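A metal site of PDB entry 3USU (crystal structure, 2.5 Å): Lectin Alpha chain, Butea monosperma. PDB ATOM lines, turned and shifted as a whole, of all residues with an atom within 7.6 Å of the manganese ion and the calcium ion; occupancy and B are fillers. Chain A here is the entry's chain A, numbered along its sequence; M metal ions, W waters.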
ATOM      1  N   ASP A  89      21.972  -3.290 -13.287  1.00  0.00           N
ATOM      2  CA  ASP A  89      20.797  -3.668 -13.977  1.00  0.00           C
ATOM      3  C   ASP A  89      20.783  -3.144 -15.412  1.00  0.00           C
ATOM      4  O   ASP A  89      20.222  -3.742 -16.239  1.00  0.00           O
ATOM      5  CB  ASP A  89      19.637  -3.171 -13.216  1.00  0.00           C
ATOM      6  CG  ASP A  89      19.110  -4.171 -12.266  1.00  0.00           C
ATOM      7  OD1 ASP A  89      19.173  -3.938 -11.078  1.00  0.00           O
ATOM      8  OD2 ASP A  89      18.658  -5.195 -12.700  1.00  0.00           O
ATOM      9  N   GLY A  90      21.429  -2.024 -15.684  1.00  0.00           N
ATOM     10  CA  GLY A  90      21.493  -1.453 -17.041  1.00  0.00           C
ATOM     11  C   GLY A  90      21.604   0.061 -17.143  1.00  0.00           C
ATOM     12  O   GLY A  90      21.867   0.747 -16.157  1.00  0.00           O
ATOM     13  N   ALA A 106      17.131  -0.276  -9.317  1.00  0.00           N
ATOM     14  CA  ALA A 106      17.229  -1.673  -9.751  1.00  0.00           C
ATOM     15  C   ALA A 106      16.858  -1.912 -11.257  1.00  0.00           C
ATOM     16  O   ALA A 106      17.119  -1.061 -12.107  1.00  0.00           O
ATOM     17  CB  ALA A 106      16.479  -2.610  -8.780  1.00  0.00           C
ATOM     18  N   GLY A 107      16.287  -3.070 -11.580  1.00  0.00           N
ATOM     19  CA  GLY A 107      15.672  -3.310 -12.916  1.00  0.00           C
ATOM     20  C   GLY A 107      14.618  -2.344 -13.487  1.00  0.00           C
ATOM     21  O   GLY A 107      14.256  -2.465 -14.671  1.00  0.00           O
ATOM     22  N   PHE A 108      14.084  -1.429 -12.659  1.00  0.00           N
ATOM     23  CA  PHE A 108      13.218  -0.352 -13.157  1.00  0.00           C
ATOM     24  C   PHE A 108      14.012   0.685 -13.896  1.00  0.00           C
ATOM     25  O   PHE A 108      13.451   1.476 -14.644  1.00  0.00           O
ATOM     26  CB  PHE A 108      12.499   0.352 -12.016  1.00  0.00           C
ATOM     27  CG  PHE A 108      11.585  -0.525 -11.269  1.00  0.00           C
ATOM     28  CD1 PHE A 108      10.312  -0.761 -11.726  1.00  0.00           C
ATOM     29  CD2 PHE A 108      12.013  -1.149 -10.119  1.00  0.00           C
ATOM     30  CE1 PHE A 108       9.478  -1.608 -11.045  1.00  0.00           C
ATOM     31  CE2 PHE A 108      11.178  -1.979  -9.421  1.00  0.00           C
ATOM     32  CZ  PHE A 108       9.901  -2.202  -9.873  1.00  0.00           C
ATOM     33  N   LEU A 109      15.325   0.684 -13.650  1.00  0.00           N
ATOM     34  CA  LEU A 109      16.297   1.442 -14.437  1.00  0.00           C
ATOM     35  C   LEU A 109      16.156   2.960 -14.264  1.00  0.00           C
ATOM     36  O   LEU A 109      16.623   3.733 -15.129  1.00  0.00           O
ATOM     37  CB  LEU A 109      16.212   1.050 -15.917  1.00  0.00           C
ATOM     38  CG  LEU A 109      16.564  -0.366 -16.345  1.00  0.00           C
ATOM     39  CD1 LEU A 109      16.391  -0.446 -17.853  1.00  0.00           C
ATOM     40  CD2 LEU A 109      17.984  -0.756 -15.954  1.00  0.00           C
ATOM     41  N   GLU A 127      16.340   0.552 -23.753  1.00  0.00           N
ATOM     42  CA  GLU A 127      17.098   0.036 -22.638  1.00  0.00           C
ATOM     43  C   GLU A 127      18.185  -0.847 -23.177  1.00  0.00           C
ATOM     44  O   GLU A 127      18.067  -1.439 -24.243  1.00  0.00           O
ATOM     45  CB  GLU A 127      16.210  -0.707 -21.638  1.00  0.00           C
ATOM     46  CG  GLU A 127      15.603  -2.015 -22.172  1.00  0.00           C
ATOM     47  CD  GLU A 127      14.683  -2.652 -21.146  1.00  0.00           C
ATOM     48  OE1 GLU A 127      13.872  -1.916 -20.537  1.00  0.00           O
ATOM     49  OE2 GLU A 127      14.820  -3.872 -20.930  1.00  0.00           O
ATOM     50  N   PHE A 128      19.258  -0.899 -22.389  1.00  0.00           N
ATOM     51  CA  PHE A 128      20.391  -1.745 -22.588  1.00  0.00           C
ATOM     52  C   PHE A 128      20.496  -2.478 -21.268  1.00  0.00           C
ATOM     53  O   PHE A 128      21.152  -1.995 -20.339  1.00  0.00           O
ATOM     54  CB  PHE A 128      21.632  -0.905 -22.836  1.00  0.00           C
ATOM     55  CG  PHE A 128      21.534  -0.027 -24.051  1.00  0.00           C
ATOM     56  CD1 PHE A 128      22.084  -0.431 -25.264  1.00  0.00           C
ATOM     57  CD2 PHE A 128      20.920   1.233 -23.985  1.00  0.00           C
ATOM     58  CE1 PHE A 128      21.992   0.385 -26.395  1.00  0.00           C
ATOM     59  CE2 PHE A 128      20.846   2.053 -25.089  1.00  0.00           C
ATOM     60  CZ  PHE A 128      21.383   1.632 -26.303  1.00  0.00           C
ATOM     61  N   ASP A 129      19.843  -3.652 -21.225  1.00  0.00           N
ATOM     62  CA  ASP A 129      19.492  -4.334 -19.994  1.00  0.00           C
ATOM     63  C   ASP A 129      20.245  -5.594 -19.678  1.00  0.00           C
ATOM     64  O   ASP A 129      20.250  -6.599 -20.430  1.00  0.00           O
ATOM     65  CB  ASP A 129      17.969  -4.553 -19.942  1.00  0.00           C
ATOM     66  CG  ASP A 129      17.512  -5.313 -18.709  1.00  0.00           C
ATOM     67  OD1 ASP A 129      16.409  -5.804 -18.765  1.00  0.00           O
ATOM     68  OD2 ASP A 129      18.225  -5.436 -17.705  1.00  0.00           O
ATOM     69  N   THR A 130      20.746  -5.602 -18.461  1.00  0.00           N
ATOM     70  CA  THR A 130      21.894  -6.420 -18.112  1.00  0.00           C
ATOM     71  C   THR A 130      21.609  -7.520 -17.049  1.00  0.00           C
ATOM     72  O   THR A 130      22.520  -8.259 -16.614  1.00  0.00           O
ATOM     73  CB  THR A 130      22.932  -5.403 -17.666  1.00  0.00           C
ATOM     74  OG1 THR A 130      24.153  -5.629 -18.353  1.00  0.00           O
ATOM     75  CG2 THR A 130      23.063  -5.354 -16.187  1.00  0.00           C
ATOM     76  N   TYR A 131      20.331  -7.637 -16.647  1.00  0.00           N
ATOM     77  CA  TYR A 131      19.908  -8.559 -15.602  1.00  0.00           C
ATOM     78  C   TYR A 131      18.485  -8.965 -15.912  1.00  0.00           C
ATOM     79  O   TYR A 131      17.649  -8.115 -16.182  1.00  0.00           O
ATOM     80  CB  TYR A 131      20.022  -7.921 -14.214  1.00  0.00           C
ATOM     81  CG  TYR A 131      19.432  -8.734 -13.058  1.00  0.00           C
ATOM     82  CD1 TYR A 131      20.198  -9.690 -12.358  1.00  0.00           C
ATOM     83  CD2 TYR A 131      18.083  -8.556 -12.658  1.00  0.00           C
ATOM     84  CE1 TYR A 131      19.659 -10.417 -11.324  1.00  0.00           C
ATOM     85  CE2 TYR A 131      17.535  -9.288 -11.614  1.00  0.00           C
ATOM     86  CZ  TYR A 131      18.340 -10.211 -10.944  1.00  0.00           C
ATOM     87  OH  TYR A 131      17.794 -10.932  -9.934  1.00  0.00           O
ATOM     88  N   GLU A 132      18.218 -10.275 -15.899  1.00  0.00           N
ATOM     89  CA  GLU A 132      16.908 -10.790 -16.238  1.00  0.00           C
ATOM     90  C   GLU A 132      15.867 -10.731 -15.081  1.00  0.00           C
ATOM     91  O   GLU A 132      15.824 -11.619 -14.214  1.00  0.00           O
ATOM     92  CB  GLU A 132      17.025 -12.233 -16.728  1.00  0.00           C
ATOM     93  CG  GLU A 132      15.757 -12.699 -17.400  1.00  0.00           C
ATOM     94  CD  GLU A 132      15.607 -14.205 -17.504  1.00  0.00           C
ATOM     95  OE1 GLU A 132      16.272 -14.971 -16.785  1.00  0.00           O
ATOM     96  OE2 GLU A 132      14.817 -14.630 -18.378  1.00  0.00           O
ATOM     97  N   ASN A 133      15.037  -9.689 -15.104  1.00  0.00           N
ATOM     98  CA  ASN A 133      13.794  -9.640 -14.346  1.00  0.00           C
ATOM     99  C   ASN A 133      12.668 -10.397 -15.072  1.00  0.00           C
ATOM    100  O   ASN A 133      12.176  -9.987 -16.135  1.00  0.00           O
ATOM    101  CB  ASN A 133      13.365  -8.195 -14.124  1.00  0.00           C
ATOM    102  CG  ASN A 133      14.478  -7.339 -13.538  1.00  0.00           C
ATOM    103  OD1 ASN A 133      14.494  -7.049 -12.322  1.00  0.00           O
ATOM    104  ND2 ASN A 133      15.416  -6.932 -14.386  1.00  0.00           N
ATOM    105  N   THR A 134      12.241 -11.496 -14.451  1.00  0.00           N
ATOM    106  CA  THR A 134      11.315 -12.383 -15.094  1.00  0.00           C
ATOM    107  C   THR A 134       9.933 -11.880 -14.897  1.00  0.00           C
ATOM    108  O   THR A 134       9.066 -12.128 -15.738  1.00  0.00           O
ATOM    109  CB  THR A 134      11.450 -13.802 -14.565  1.00  0.00           C
ATOM    110  OG1 THR A 134      11.310 -13.782 -13.149  1.00  0.00           O
ATOM    111  CG2 THR A 134      12.834 -14.343 -14.936  1.00  0.00           C
ATOM    112  N   PHE A 136       9.550  -8.837 -15.261  1.00  0.00           N
ATOM    113  CA  PHE A 136       9.443  -7.865 -16.369  1.00  0.00           C
ATOM    114  C   PHE A 136       9.492  -8.533 -17.735  1.00  0.00           C
ATOM    115  O   PHE A 136       9.615  -7.836 -18.736  1.00  0.00           O
ATOM    116  CB  PHE A 136      10.482  -6.725 -16.333  1.00  0.00           C
ATOM    117  CG  PHE A 136      10.572  -5.986 -15.024  1.00  0.00           C
ATOM    118  CD1 PHE A 136       9.461  -5.885 -14.159  1.00  0.00           C
ATOM    119  CD2 PHE A 136      11.774  -5.377 -14.630  1.00  0.00           C
ATOM    120  CE1 PHE A 136       9.557  -5.206 -12.923  1.00  0.00           C
ATOM    121  CE2 PHE A 136      11.863  -4.719 -13.401  1.00  0.00           C
ATOM    122  CZ  PHE A 136      10.753  -4.636 -12.554  1.00  0.00           C
ATOM    123  N   LEU A 137       9.349  -9.862 -17.795  1.00  0.00           N
ATOM    124  CA  LEU A 137       9.325 -10.588 -19.073  1.00  0.00           C
ATOM    125  C   LEU A 137      10.663 -10.479 -19.833  1.00  0.00           C
ATOM    126  O   LEU A 137      10.718 -10.594 -21.051  1.00  0.00           O
ATOM    127  CB  LEU A 137       8.131 -10.155 -19.942  1.00  0.00           C
ATOM    128  CG  LEU A 137       6.694 -10.190 -19.377  1.00  0.00           C
ATOM    129  CD1 LEU A 137       5.708 -10.200 -20.524  1.00  0.00           C
ATOM    130  CD2 LEU A 137       6.401 -11.345 -18.416  1.00  0.00           C
ATOM    131  N   ASP A 138      11.721 -10.249 -19.067  1.00  0.00           N
ATOM    132  CA  ASP A 138      13.052 -10.186 -19.551  1.00  0.00           C
ATOM    133  C   ASP A 138      13.488 -11.501 -20.125  1.00  0.00           C
ATOM    134  O   ASP A 138      13.207 -12.557 -19.539  1.00  0.00           O
ATOM    135  CB  ASP A 138      14.014  -9.899 -18.415  1.00  0.00           C
ATOM    136  CG  ASP A 138      14.365  -8.457 -18.322  1.00  0.00           C
ATOM    137  OD1 ASP A 138      14.180  -7.728 -19.309  1.00  0.00           O
ATOM    138  OD2 ASP A 138      14.841  -8.026 -17.254  1.00  0.00           O
ATOM    139  N   PRO A 139      14.210 -11.450 -21.239  1.00  0.00           N
ATOM    140  CA  PRO A 139      14.810 -12.624 -21.805  1.00  0.00           C
ATOM    141  C   PRO A 139      16.078 -12.974 -21.009  1.00  0.00           C
ATOM    142  O   PRO A 139      16.697 -12.090 -20.388  1.00  0.00           O
ATOM    143  CB  PRO A 139      15.094 -12.213 -23.244  1.00  0.00           C
ATOM    144  CG  PRO A 139      15.290 -10.734 -23.213  1.00  0.00           C
ATOM    145  CD  PRO A 139      14.514 -10.222 -22.007  1.00  0.00           C
ATOM    146  N   ASP A 141      19.077 -13.583 -21.741  1.00  0.00           N
ATOM    147  CA  ASP A 141      20.303 -12.946 -22.179  1.00  0.00           C
ATOM    148  C   ASP A 141      20.218 -11.440 -22.026  1.00  0.00           C
ATOM    149  O   ASP A 141      19.138 -10.886 -22.023  1.00  0.00           O
ATOM    150  CB  ASP A 141      20.498 -13.277 -23.652  1.00  0.00           C
ATOM    151  CG  ASP A 141      19.288 -12.853 -24.500  1.00  0.00           C
ATOM    152  OD1 ASP A 141      19.362 -11.709 -25.038  1.00  0.00           O
ATOM    153  OD2 ASP A 141      18.269 -13.616 -24.570  1.00  0.00           O
ATOM    154  N   HIS A 143      20.356  -7.785 -23.357  1.00  0.00           N
ATOM    155  CA  HIS A 143      19.508  -7.430 -24.507  1.00  0.00           C
ATOM    156  C   HIS A 143      19.312  -5.952 -24.597  1.00  0.00           C
ATOM    157  O   HIS A 143      19.532  -5.235 -23.621  1.00  0.00           O
ATOM    158  CB  HIS A 143      18.142  -8.095 -24.435  1.00  0.00           C
ATOM    159  CG  HIS A 143      17.356  -7.741 -23.187  1.00  0.00           C
ATOM    160  ND1 HIS A 143      17.774  -8.055 -21.971  1.00  0.00           N
ATOM    161  CD2 HIS A 143      16.147  -7.082 -23.025  1.00  0.00           C
ATOM    162  CE1 HIS A 143      16.872  -7.631 -21.070  1.00  0.00           C
ATOM    163  NE2 HIS A 143      15.896  -7.019 -21.711  1.00  0.00           N
ATOM    164  N   ILE A 144      18.981  -5.482 -25.791  1.00  0.00           N
ATOM    165  CA  ILE A 144      18.625  -4.086 -26.004  1.00  0.00           C
ATOM    166  C   ILE A 144      17.109  -4.137 -26.130  1.00  0.00           C
ATOM    167  O   ILE A 144      16.594  -5.012 -26.829  1.00  0.00           O
ATOM    168  CB  ILE A 144      19.247  -3.572 -27.300  1.00  0.00           C
ATOM    169  CG1 ILE A 144      20.719  -3.274 -27.099  1.00  0.00           C
ATOM    170  CG2 ILE A 144      18.552  -2.310 -27.781  1.00  0.00           C
ATOM    171  CD1 ILE A 144      21.552  -3.480 -28.354  1.00  0.00           C
ATOM    172  N   GLY A 145      16.413  -3.241 -25.437  1.00  0.00           N
ATOM    173  CA  GLY A 145      14.961  -3.179 -25.464  1.00  0.00           C
ATOM    174  C   GLY A 145      14.493  -1.843 -26.016  1.00  0.00           C
ATOM    175  O   GLY A 145      15.224  -0.871 -25.906  1.00  0.00           O
ATOM    176  N   ASP A 147      11.249   0.431 -25.028  1.00  0.00           N
ATOM    177  CA  ASP A 147      10.213   0.471 -23.955  1.00  0.00           C
ATOM    178  C   ASP A 147       9.310   1.678 -24.106  1.00  0.00           C
ATOM    179  O   ASP A 147       9.797   2.784 -24.202  1.00  0.00           O
ATOM    180  CB  ASP A 147      10.848   0.624 -22.567  1.00  0.00           C
ATOM    181  CG  ASP A 147      11.768  -0.498 -22.183  1.00  0.00           C
ATOM    182  OD1 ASP A 147      11.677  -1.607 -22.712  1.00  0.00           O
ATOM    183  OD2 ASP A 147      12.624  -0.265 -21.299  1.00  0.00           O
ATOM    184  N   ILE A 151       8.261  -1.290 -18.314  1.00  0.00           N
ATOM    185  CA  ILE A 151       9.586  -1.924 -18.270  1.00  0.00           C
ATOM    186  C   ILE A 151       9.663  -3.219 -19.132  1.00  0.00           C
ATOM    187  O   ILE A 151      10.751  -3.705 -19.506  1.00  0.00           O
ATOM    188  CB  ILE A 151      10.050  -2.112 -16.807  1.00  0.00           C
ATOM    189  CG1 ILE A 151      11.554  -2.374 -16.706  1.00  0.00           C
ATOM    190  CG2 ILE A 151       9.272  -3.226 -16.122  1.00  0.00           C
ATOM    191  CD1 ILE A 151      12.453  -1.227 -17.128  1.00  0.00           C
ATOM    192  N   LYS A 152       8.468  -3.752 -19.423  1.00  0.00           N
ATOM    193  CA  LYS A 152       8.300  -4.885 -20.283  1.00  0.00           C
ATOM    194  C   LYS A 152       8.415  -4.295 -21.638  1.00  0.00           C
ATOM    195  O   LYS A 152       7.443  -3.799 -22.193  1.00  0.00           O
ATOM    196  CB  LYS A 152       6.925  -5.528 -20.090  1.00  0.00           C
ATOM    197  CG  LYS A 152       6.553  -5.821 -18.636  1.00  0.00           C
ATOM    198  CD  LYS A 152       5.141  -6.374 -18.568  1.00  0.00           C
ATOM    199  CE  LYS A 152       5.077  -7.612 -17.684  1.00  0.00           C
ATOM    200  NZ  LYS A 152       3.831  -7.606 -16.861  1.00  0.00           N
ATOM    201  N   SER A 153       9.645  -4.335 -22.158  1.00  0.00           N
ATOM    202  CA  SER A 153       9.958  -3.984 -23.523  1.00  0.00           C
ATOM    203  C   SER A 153       8.943  -4.560 -24.491  1.00  0.00           C
ATOM    204  O   SER A 153       8.460  -5.670 -24.305  1.00  0.00           O
ATOM    205  CB  SER A 153      11.327  -4.526 -23.878  1.00  0.00           C
ATOM    206  OG  SER A 153      12.303  -4.143 -22.899  1.00  0.00           O
ATOM    207  N   THR A 156      12.606  -6.708 -27.985  1.00  0.00           N
ATOM    208  CA  THR A 156      13.981  -6.800 -27.565  1.00  0.00           C
ATOM    209  C   THR A 156      14.841  -7.491 -28.642  1.00  0.00           C
ATOM    210  O   THR A 156      14.329  -8.029 -29.605  1.00  0.00           O
ATOM    211  CB  THR A 156      14.093  -7.538 -26.222  1.00  0.00           C
ATOM    212  OG1 THR A 156      13.911  -8.937 -26.457  1.00  0.00           O
ATOM    213  CG2 THR A 156      13.049  -7.044 -25.209  1.00  0.00           C
HETATM  214 MN    MN M   1      14.631  -5.715 -20.190  1.00  0.00          MN
HETATM  215 CA    CA M   2      16.112  -6.252 -16.383  1.00  0.00          CA
HETATM  216  O   HOH W   1      14.702  -4.844 -16.809  1.00  0.00           O
HETATM  217  O   HOH W   2      12.984  -6.037 -21.706  1.00  0.00           O
HETATM  218  O   HOH W   3      13.049  -4.411 -18.757  1.00  0.00           O
HETATM  219  O   HOH W   4      17.417  -4.925 -15.279  1.00  0.00           O
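The calcium ion is bound by water W1. Water W4 binds the calcium ion (2.2 Å). The calcium ion is bound by ND2 of Asn 133. The side-chain carboxylate (OD2) of Asp 138 is bound to the calcium ion, 2.3 Å away. The calcium ion is bound by O of Tyr 131, at 2.4 Å. OD1 of Asp 129 is bound to the calcium ion, at 2.4 Å. The calcium ion is bound by OD2 of Asp 129, 2.6 Å away. The calcium ion has seven donor atoms within binding distance.
Within 4 Å of the calcium ion: Asp 129, Tyr 131, Asn 133 and Asp 138. Along chain A the residues within 4 Å of the calcium ion span positions 129 to 138. The nearest printed residue that does not touch the calcium ion is Gly 107 (4.6 Å).
ND1 of His 143 sits at hydrogen-bond distance from O of Asp 141. OD1 of Asp 147 lies within hydrogen-bond range of OG of Ser 153, 2.6 Å away. OE2 of Glu 127 lies close to OG of Ser 153, at 3.2 Å. The backbone NH (N) of Gly 145 sits at hydrogen-bond distance from the backbone carbonyl oxygen (O) of Glu 127 (2.7 Å).
The manganese ion is bound by OE2 of Glu 127 (2.0 Å). The manganese ion is bound by OD1 of Asp 138 (2.2 Å). Water W2 binds the manganese ion, 2.3 Å away. OD1 of Asp 129 is bound to the manganese ion, 2.3 Å away. The manganese ion is bound by NE2 of His 143, at 2.4 Å. Water W3 is bound to the manganese ion (2.5 Å).
Water W3 bridges O of Ile 151 and OE1 of Glu 127.
Ser 153 touches the manganese ion (OG to MN, 3.9 Å). Within 4 Å of the manganese ion: Glu 127, Asp 129, Asp 138, His 143 and Ser 153. Along chain A the residues within 4 Å of the manganese ion span positions 127 to 153. The nearest printed residue that does not touch the manganese ion is Ile 151 (4.4 Å).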
